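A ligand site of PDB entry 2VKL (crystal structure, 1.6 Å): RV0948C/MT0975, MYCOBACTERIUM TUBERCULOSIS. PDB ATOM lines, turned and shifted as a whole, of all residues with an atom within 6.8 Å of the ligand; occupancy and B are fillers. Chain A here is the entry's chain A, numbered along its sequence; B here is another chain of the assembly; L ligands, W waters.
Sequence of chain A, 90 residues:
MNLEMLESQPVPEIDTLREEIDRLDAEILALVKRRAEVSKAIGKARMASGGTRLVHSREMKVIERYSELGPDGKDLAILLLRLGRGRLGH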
ATOM      1  N   ARG A  35     -25.966   8.411  12.529  1.00  0.00           N
ATOM      2  CA  ARG A  35     -25.045   8.879  13.595  1.00  0.00           C
ATOM      3  C   ARG A  35     -24.244   7.689  14.214  1.00  0.00           C
ATOM      4  O   ARG A  35     -23.041   7.786  14.459  1.00  0.00           O
ATOM      5  CB  ARG A  35     -25.805   9.585  14.698  1.00  0.00           C
ATOM      6  CG  ARG A  35     -24.858  10.445  15.595  1.00  0.00           C
ATOM      7  CD  ARG A  35     -25.537  10.748  16.939  1.00  0.00           C
ATOM      8  NE  ARG A  35     -24.851  11.793  17.676  1.00  0.00           N
ATOM      9  CZ  ARG A  35     -23.749  11.593  18.376  1.00  0.00           C
ATOM     10  NH1 ARG A  35     -23.198  10.381  18.417  1.00  0.00           N
ATOM     11  NH2 ARG A  35     -23.165  12.622  18.990  1.00  0.00           N
ATOM     12  N   VAL A  38     -21.461   6.648  11.902  1.00  0.00           N
ATOM     13  CA  VAL A  38     -20.348   7.613  11.892  1.00  0.00           C
ATOM     14  C   VAL A  38     -19.545   7.502  13.206  1.00  0.00           C
ATOM     15  O   VAL A  38     -18.318   7.463  13.201  1.00  0.00           O
ATOM     16  CB  VAL A  38     -20.808   9.042  11.698  1.00  0.00           C
ATOM     17  CG1 VAL A  38     -19.602  10.035  11.802  1.00  0.00           C
ATOM     18  CG2 VAL A  38     -21.560   9.172  10.337  1.00  0.00           C
ATOM     19  N   SER A  39     -20.272   7.413  14.317  1.00  0.00           N
ATOM     20  CA  SER A  39     -19.676   7.216  15.650  1.00  0.00           C
ATOM     21  C   SER A  39     -18.791   5.957  15.720  1.00  0.00           C
ATOM     22  O   SER A  39     -17.688   6.015  16.251  1.00  0.00           O
ATOM     23  CB  SER A  39     -20.765   7.125  16.714  1.00  0.00           C
ATOM     24  OG  SER A  39     -21.393   8.355  16.849  1.00  0.00           O
ATOM     25  N   LYS A  40     -19.294   4.863  15.174  1.00  0.00           N
ATOM     26  CA  LYS A  40     -18.553   3.587  15.180  1.00  0.00           C
ATOM     27  C   LYS A  40     -17.268   3.725  14.378  1.00  0.00           C
ATOM     28  O   LYS A  40     -16.215   3.213  14.786  1.00  0.00           O
ATOM     29  CB  LYS A  40     -19.448   2.462  14.659  1.00  0.00           C
ATOM     30  CG  LYS A  40     -20.465   1.989  15.678  1.00  0.00           C
ATOM     31  CD  LYS A  40     -21.465   1.044  15.041  1.00  0.00           C
ATOM     32  CE  LYS A  40     -22.480   0.646  16.015  1.00  0.00           C
ATOM     33  NZ  LYS A  40     -23.336  -0.380  15.398  1.00  0.00           N
ATOM     34  N   ILE A  42     -15.591   6.530  13.820  1.00  0.00           N
ATOM     35  CA  ILE A  42     -14.660   7.308  14.645  1.00  0.00           C
ATOM     36  C   ILE A  42     -13.977   6.442  15.688  1.00  0.00           C
ATOM     37  O   ILE A  42     -12.748   6.524  15.875  1.00  0.00           O
ATOM     38  CB  ILE A  42     -15.401   8.456  15.376  1.00  0.00           C
ATOM     39  CG1 ILE A  42     -15.837   9.496  14.339  1.00  0.00           C
ATOM     40  CG2 ILE A  42     -14.469   9.063  16.438  1.00  0.00           C
ATOM     41  CD1 ILE A  42     -16.887  10.453  14.856  1.00  0.00           C
ATOM     42  N   GLY A  43     -14.754   5.641  16.395  1.00  0.00           N
ATOM     43  CA  GLY A  43     -14.260   4.749  17.441  1.00  0.00           C
ATOM     44  C   GLY A  43     -13.176   3.825  16.901  1.00  0.00           C
ATOM     45  O   GLY A  43     -12.091   3.714  17.502  1.00  0.00           O
ATOM     46  N   ARG A  46      -9.993   5.743  15.870  1.00  0.00           N
ATOM     47  CA  ARG A  46      -9.301   6.207  17.070  1.00  0.00           C
ATOM     48  C   ARG A  46      -8.507   5.075  17.708  1.00  0.00           C
ATOM     49  O   ARG A  46      -7.311   5.206  18.015  1.00  0.00           O
ATOM     50  CB  ARG A  46     -10.335   6.774  18.062  1.00  0.00           C
ATOM     51  CG  ARG A  46      -9.720   7.409  19.311  1.00  0.00           C
ATOM     52  CD  ARG A  46     -10.759   8.122  20.180  1.00  0.00           C
ATOM     53  NE  ARG A  46     -11.774   7.228  20.735  1.00  0.00           N
ATOM     54  CZ  ARG A  46     -11.558   6.353  21.715  1.00  0.00           C
ATOM     55  NH1 ARG A  46     -10.330   6.179  22.227  1.00  0.00           N
ATOM     56  NH2 ARG A  46     -12.555   5.617  22.166  1.00  0.00           N
ATOM     57  N   THR A  52      -6.622   9.119  21.926  1.00  0.00           N
ATOM     58  CA  THR A  52      -7.203   9.305  23.219  1.00  0.00           C
ATOM     59  C   THR A  52      -8.691   9.646  23.100  1.00  0.00           C
ATOM     60  O   THR A  52      -9.099  10.434  22.245  1.00  0.00           O
ATOM     61  CB  THR A  52      -6.410  10.366  24.009  1.00  0.00           C
ATOM     62  OG1 THR A  52      -5.063   9.857  24.217  1.00  0.00           O
ATOM     63  CG2 THR A  52      -7.089  10.669  25.353  1.00  0.00           C
ATOM     64  N   ARG A  53      -9.499   9.043  23.968  1.00  0.00           N
ATOM     65  CA  ARG A  53     -10.910   9.338  23.981  1.00  0.00           C
ATOM     66  C   ARG A  53     -11.149  10.738  24.480  1.00  0.00           C
ATOM     67  O   ARG A  53     -10.594  11.124  25.496  1.00  0.00           O
ATOM     68  CB  ARG A  53     -11.656   8.345  24.880  1.00  0.00           C
ATOM     69  CG  ARG A  53     -13.156   8.521  24.785  1.00  0.00           C
ATOM     70  CD  ARG A  53     -13.863   7.461  25.602  1.00  0.00           C
ATOM     71  NE  ARG A  53     -15.235   7.824  25.857  1.00  0.00           N
ATOM     72  CZ  ARG A  53     -16.049   7.210  26.706  1.00  0.00           C
ATOM     73  NH1 ARG A  53     -15.623   6.163  27.399  1.00  0.00           N
ATOM     74  NH2 ARG A  53     -17.285   7.651  26.856  1.00  0.00           N
ATOM     75  N   LEU A  54     -12.001  11.487  23.786  1.00  0.00           N
ATOM     76  CA  LEU A  54     -12.253  12.882  24.113  1.00  0.00           C
ATOM     77  C   LEU A  54     -13.450  13.097  25.047  1.00  0.00           C
ATOM     78  O   LEU A  54     -14.425  13.772  24.706  1.00  0.00           O
ATOM     79  CB  LEU A  54     -12.363  13.716  22.834  1.00  0.00           C
ATOM     80  CG  LEU A  54     -11.169  13.650  21.879  1.00  0.00           C
ATOM     81  CD1 LEU A  54     -11.387  14.574  20.680  1.00  0.00           C
ATOM     82  CD2 LEU A  54      -9.884  13.964  22.634  1.00  0.00           C
ATOM     83  N   ARG A  58     -14.756  16.936  23.884  1.00  0.00           N
ATOM     84  CA  ARG A  58     -15.808  16.744  22.858  1.00  0.00           C
ATOM     85  C   ARG A  58     -17.091  16.074  23.381  1.00  0.00           C
ATOM     86  O   ARG A  58     -18.202  16.555  23.132  1.00  0.00           O
ATOM     87  CB  ARG A  58     -15.244  15.984  21.691  1.00  0.00           C
ATOM     88  CG  ARG A  58     -16.270  15.783  20.672  1.00  0.00           C
ATOM     89  CD  ARG A  58     -15.685  15.559  19.346  1.00  0.00           C
ATOM     90  NE  ARG A  58     -16.768  15.074  18.548  1.00  0.00           N
ATOM     91  CZ  ARG A  58     -17.635  15.841  17.927  1.00  0.00           C
ATOM     92  NH1 ARG A  58     -18.639  15.270  17.281  1.00  0.00           N
ATOM     93  NH2 ARG A  58     -17.468  17.151  17.894  1.00  0.00           N
ATOM     94  N   GLU A  59     -16.958  14.955  24.081  1.00  0.00           N
ATOM     95  CA  GLU A  59     -18.184  14.271  24.573  1.00  0.00           C
ATOM     96  C   GLU A  59     -18.990  15.176  25.521  1.00  0.00           C
ATOM     97  O   GLU A  59     -20.220  15.236  25.458  1.00  0.00           O
ATOM     98  CB  GLU A  59     -17.850  12.926  25.190  1.00  0.00           C
ATOM     99  CG  GLU A  59     -17.167  11.985  24.167  1.00  0.00           C
ATOM    100  CD  GLU A  59     -16.983  10.575  24.686  1.00  0.00           C
ATOM    101  OE1 GLU A  59     -17.564  10.218  25.743  1.00  0.00           O
ATOM    102  OE2 GLU A  59     -16.198   9.822  24.072  1.00  0.00           O
ATOM    103  N   VAL A  62     -20.969  17.522  23.431  1.00  0.00           N
ATOM    104  CA  VAL A  62     -22.203  16.853  22.864  1.00  0.00           C
ATOM    105  C   VAL A  62     -23.289  16.829  23.949  1.00  0.00           C
ATOM    106  O   VAL A  62     -24.427  17.181  23.688  1.00  0.00           O
ATOM    107  CB  VAL A  62     -21.907  15.437  22.388  1.00  0.00           C
ATOM    108  CG1 VAL A  62     -23.191  14.642  22.024  1.00  0.00           C
ATOM    109  CG2 VAL A  62     -20.855  15.500  21.177  1.00  0.00           C
ATOM    110  N   ALA A  77     -27.986  12.494  24.959  1.00  0.00           N
ATOM    111  CA  ALA A  77     -26.572  12.559  24.502  1.00  0.00           C
ATOM    112  C   ALA A  77     -25.748  11.301  24.909  1.00  0.00           C
ATOM    113  O   ALA A  77     -25.012  10.724  24.123  1.00  0.00           O
ATOM    114  CB  ALA A  77     -25.893  13.800  25.054  1.00  0.00           C
ATOM    115  N   LEU A  80     -26.725   8.423  22.780  1.00  0.00           N
ATOM    116  CA  LEU A  80     -26.169   8.549  21.393  1.00  0.00           C
ATOM    117  C   LEU A  80     -24.685   8.210  21.396  1.00  0.00           C
ATOM    118  O   LEU A  80     -24.199   7.537  20.521  1.00  0.00           O
ATOM    119  CB  LEU A  80     -26.419   9.932  20.803  1.00  0.00           C
ATOM    120  CG  LEU A  80     -27.915  10.276  20.586  1.00  0.00           C
ATOM    121  CD1 LEU A  80     -28.022  11.739  20.110  1.00  0.00           C
ATOM    122  CD2 LEU A  80     -28.581   9.305  19.605  1.00  0.00           C
ATOM    123  N   LEU A  81     -23.959   8.670  22.426  1.00  0.00           N
ATOM    124  CA  LEU A  81     -22.538   8.292  22.516  1.00  0.00           C
ATOM    125  C   LEU A  81     -22.398   6.781  22.661  1.00  0.00           C
ATOM    126  O   LEU A  81     -21.522   6.178  22.029  1.00  0.00           O
ATOM    127  CB  LEU A  81     -21.890   9.032  23.672  1.00  0.00           C
ATOM    128  CG  LEU A  81     -21.763  10.555  23.450  1.00  0.00           C
ATOM    129  CD1 LEU A  81     -21.614  11.347  24.777  1.00  0.00           C
ATOM    130  CD2 LEU A  81     -20.631  10.922  22.468  1.00  0.00           C
ATOM    131  N   ARG A  82     -23.250   6.173  23.487  1.00  0.00           N
ATOM    132  CA  ARG A  82     -23.238   4.706  23.727  1.00  0.00           C
ATOM    133  C   ARG A  82     -23.477   3.916  22.447  1.00  0.00           C
ATOM    134  O   ARG A  82     -22.815   2.882  22.198  1.00  0.00           O
ATOM    135  CB  ARG A  82     -24.303   4.302  24.730  1.00  0.00           C
ATOM    136  CG  ARG A  82     -23.958   4.660  26.133  1.00  0.00           C
ATOM    137  CD  ARG A  82     -25.058   4.323  27.069  1.00  0.00           C
ATOM    138  NE  ARG A  82     -24.746   4.759  28.441  1.00  0.00           N
ATOM    139  CZ  ARG A  82     -25.394   4.320  29.519  1.00  0.00           C
ATOM    140  NH1 ARG A  82     -26.389   3.462  29.394  1.00  0.00           N
ATOM    141  NH2 ARG A  82     -25.026   4.756  30.727  1.00  0.00           N
ATOM    142  N   GLY A  84     -22.546   4.616  19.646  1.00  0.00           N
ATOM    143  CA  GLY A  84     -21.298   4.608  18.896  1.00  0.00           C
ATOM    144  C   GLY A  84     -20.243   3.619  19.353  1.00  0.00           C
ATOM    145  O   GLY A  84     -19.261   3.395  18.635  1.00  0.00           O
ATOM    146  N   ARG A  85     -20.422   3.019  20.521  1.00  0.00           N
ATOM    147  CA  ARG A  85     -19.323   2.316  21.174  1.00  0.00           C
ATOM    148  C   ARG A  85     -19.335   0.790  21.080  1.00  0.00           C
ATOM    149  O   ARG A  85     -18.424   0.129  21.601  1.00  0.00           O
ATOM    150  CB  ARG A  85     -19.215   2.784  22.638  1.00  0.00           C
ATOM    151  CG  ARG A  85     -18.555   4.156  22.728  1.00  0.00           C
ATOM    152  CD  ARG A  85     -17.895   4.426  24.067  1.00  0.00           C
ATOM    153  NE  ARG A  85     -18.862   4.402  25.173  1.00  0.00           N
ATOM    154  CZ  ARG A  85     -19.672   5.422  25.533  1.00  0.00           C
ATOM    155  NH1 ARG A  85     -19.657   6.557  24.880  1.00  0.00           N
ATOM    156  NH2 ARG A  85     -20.492   5.295  26.571  1.00  0.00           N
ATOM    157  N   ILE B  14     -10.695  11.505  10.775  1.00  0.00           N
ATOM    158  CA  ILE B  14     -11.508  11.335  11.950  1.00  0.00           C
ATOM    159  C   ILE B  14     -12.197  12.650  12.310  1.00  0.00           C
ATOM    160  O   ILE B  14     -13.387  12.680  12.680  1.00  0.00           O
ATOM    161  CB  ILE B  14     -10.648  10.727  13.101  1.00  0.00           C
ATOM    162  CG1 ILE B  14     -11.523  10.150  14.201  1.00  0.00           C
ATOM    163  CG2 ILE B  14      -9.635  11.758  13.642  1.00  0.00           C
ATOM    164  CD1 ILE B  14     -10.737   9.292  15.225  1.00  0.00           C
ATOM    165  N   ARG B  18     -16.140  13.800  12.746  1.00  0.00           N
ATOM    166  CA  ARG B  18     -16.665  14.511  13.932  1.00  0.00           C
ATOM    167  C   ARG B  18     -17.494  15.715  13.503  1.00  0.00           C
ATOM    168  O   ARG B  18     -18.559  15.975  14.070  1.00  0.00           O
ATOM    169  CB  ARG B  18     -15.533  14.890  14.887  1.00  0.00           C
ATOM    170  CG  ARG B  18     -15.004  13.699  15.689  1.00  0.00           C
ATOM    171  CD  ARG B  18     -13.803  14.046  16.556  1.00  0.00           C
ATOM    172  NE  ARG B  18     -13.547  12.934  17.482  1.00  0.00           N
ATOM    173  CZ  ARG B  18     -12.380  12.326  17.650  1.00  0.00           C
ATOM    174  NH1 ARG B  18     -11.281  12.690  16.983  1.00  0.00           N
ATOM    175  NH2 ARG B  18     -12.330  11.332  18.519  1.00  0.00           N
ATOM    176  N   ILE B  21     -20.826  14.411  12.698  1.00  0.00           N
ATOM    177  CA  ILE B  21     -21.584  14.103  13.913  1.00  0.00           C
ATOM    178  C   ILE B  21     -22.292  15.365  14.354  1.00  0.00           C
ATOM    179  O   ILE B  21     -23.477  15.368  14.727  1.00  0.00           O
ATOM    180  CB  ILE B  21     -20.728  13.515  15.050  1.00  0.00           C
ATOM    181  CG1 ILE B  21     -20.263  12.088  14.754  1.00  0.00           C
ATOM    182  CG2 ILE B  21     -21.503  13.576  16.374  1.00  0.00           C
ATOM    183  CD1 ILE B  21     -21.341  11.056  14.831  1.00  0.00           C
ATOM    184  N   ASP B  22     -21.579  16.460  14.323  1.00  0.00           N
ATOM    185  CA  ASP B  22     -22.129  17.728  14.843  1.00  0.00           C
ATOM    186  C   ASP B  22     -23.293  18.198  13.998  1.00  0.00           C
ATOM    187  O   ASP B  22     -24.291  18.739  14.522  1.00  0.00           O
ATOM    188  CB  ASP B  22     -21.057  18.812  14.930  1.00  0.00           C
ATOM    189  CG  ASP B  22     -20.021  18.531  16.018  1.00  0.00           C
ATOM    190  OD1 ASP B  22     -18.971  19.222  16.046  1.00  0.00           O
ATOM    191  OD2 ASP B  22     -20.240  17.652  16.853  1.00  0.00           O
ATOM    192  N   ASP B  25     -26.213  15.901  14.816  1.00  0.00           N
ATOM    193  CA  ASP B  25     -26.798  16.317  16.108  1.00  0.00           C
ATOM    194  C   ASP B  25     -27.723  17.559  15.944  1.00  0.00           C
ATOM    195  O   ASP B  25     -28.790  17.652  16.579  1.00  0.00           O
ATOM    196  CB  ASP B  25     -25.718  16.585  17.132  1.00  0.00           C
ATOM    197  CG  ASP B  25     -25.171  15.290  17.722  1.00  0.00           C
ATOM    198  OD1 ASP B  25     -24.013  15.309  18.205  1.00  0.00           O
ATOM    199  OD2 ASP B  25     -25.926  14.257  17.733  1.00  0.00           O
HETATM  200  C1  LIG L   1     -19.817  10.891  19.126  1.00  0.00           C
HETATM  201  O1  LIG L   1     -20.153   9.682  19.166  1.00  0.00           O
HETATM  202  O2  LIG L   1     -20.581  11.765  19.469  1.00  0.00           O
HETATM  203  C2  LIG L   1     -18.484  11.430  18.725  1.00  0.00           C
HETATM  204  O3  LIG L   1     -18.528  12.867  19.030  1.00  0.00           O
HETATM  205  C3  LIG L   1     -17.433  10.661  19.511  1.00  0.00           C
HETATM  206  C4  LIG L   1     -16.018  11.200  19.253  1.00  0.00           C
HETATM  207  O4  LIG L   1     -15.023  10.549  19.664  1.00  0.00           O
HETATM  208  O5  LIG L   1     -15.791  12.236  18.610  1.00  0.00           O
HETATM  209  O   HOH W   1     -14.159  10.505  22.276  1.00  0.00           O
HETATM  210  O   HOH W   2     -14.544   7.913  19.727  1.00  0.00           O
HETATM  211  O   HOH W   3     -19.395   7.397  20.530  1.00  0.00           O
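Water W2 bridges O4 of the ligand (2.7 Å) and NE of Arg 46 (3.0 Å).
Water W1 lies within hydrogen-bond range of O4 of the ligand (2.8 Å), OE2 of Glu 59 (2.8 Å) and N of Leu 54 (2.8 Å).
Water W3 bridges an oxygen (O1) of the ligand (2.8 Å) and the backbone carbonyl oxygen of Leu 81 (2.9 Å).
Ile 42 touches the ligand (CG2 to O4, 3.6 Å).
Leu 81 touches the ligand.
Ile 21 of chain B touches the ligand (CG2 to O2, 3.7 Å).
Hydrophobic or aromatic side chains that line the ligand: Ile 42, Leu 81 and Ile 21 of chain B.
Of the 24 residues printed, 7 come within 4 Å of the ligand.
The nearest printed residue that does not touch the ligand is Val 62 (4.1 Å).
The guanidinium group (NE) of Arg 18 of chain B is in salt-bridge range of an oxygen (O5) of the ligand, 2.6 Å away.
The guanidinium group (NH2) of Arg 35 lies within salt-bridge range of an oxygen (O2) of the ligand, at 2.8 Å.
An oxygen (O5) of the ligand is in salt-bridge range of the guanidinium group (NE) of Arg 58 (3.0 Å).
OG of Ser 39 is in hydrogen-bond range of O1 of the ligand (2.9 Å).
O of Arg 18 of chain B is in hydrogen-bond range of NH1 of Arg 58, at 3.3 Å.
OG of Ser 39 is in hydrogen-bond range of O of Arg 35.
NE of Arg 35 lies within salt-bridge range of OD2 of Asp 25 of chain B, 2.7 Å away.
The guanidinium group (NH1) of Arg 58 lies within salt-bridge range of the side-chain carboxylate (OD2) of Asp 22 of chain B.
O of Leu 81 sits at hydrogen-bond distance from NH1 of Arg 85 (3.4 Å).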
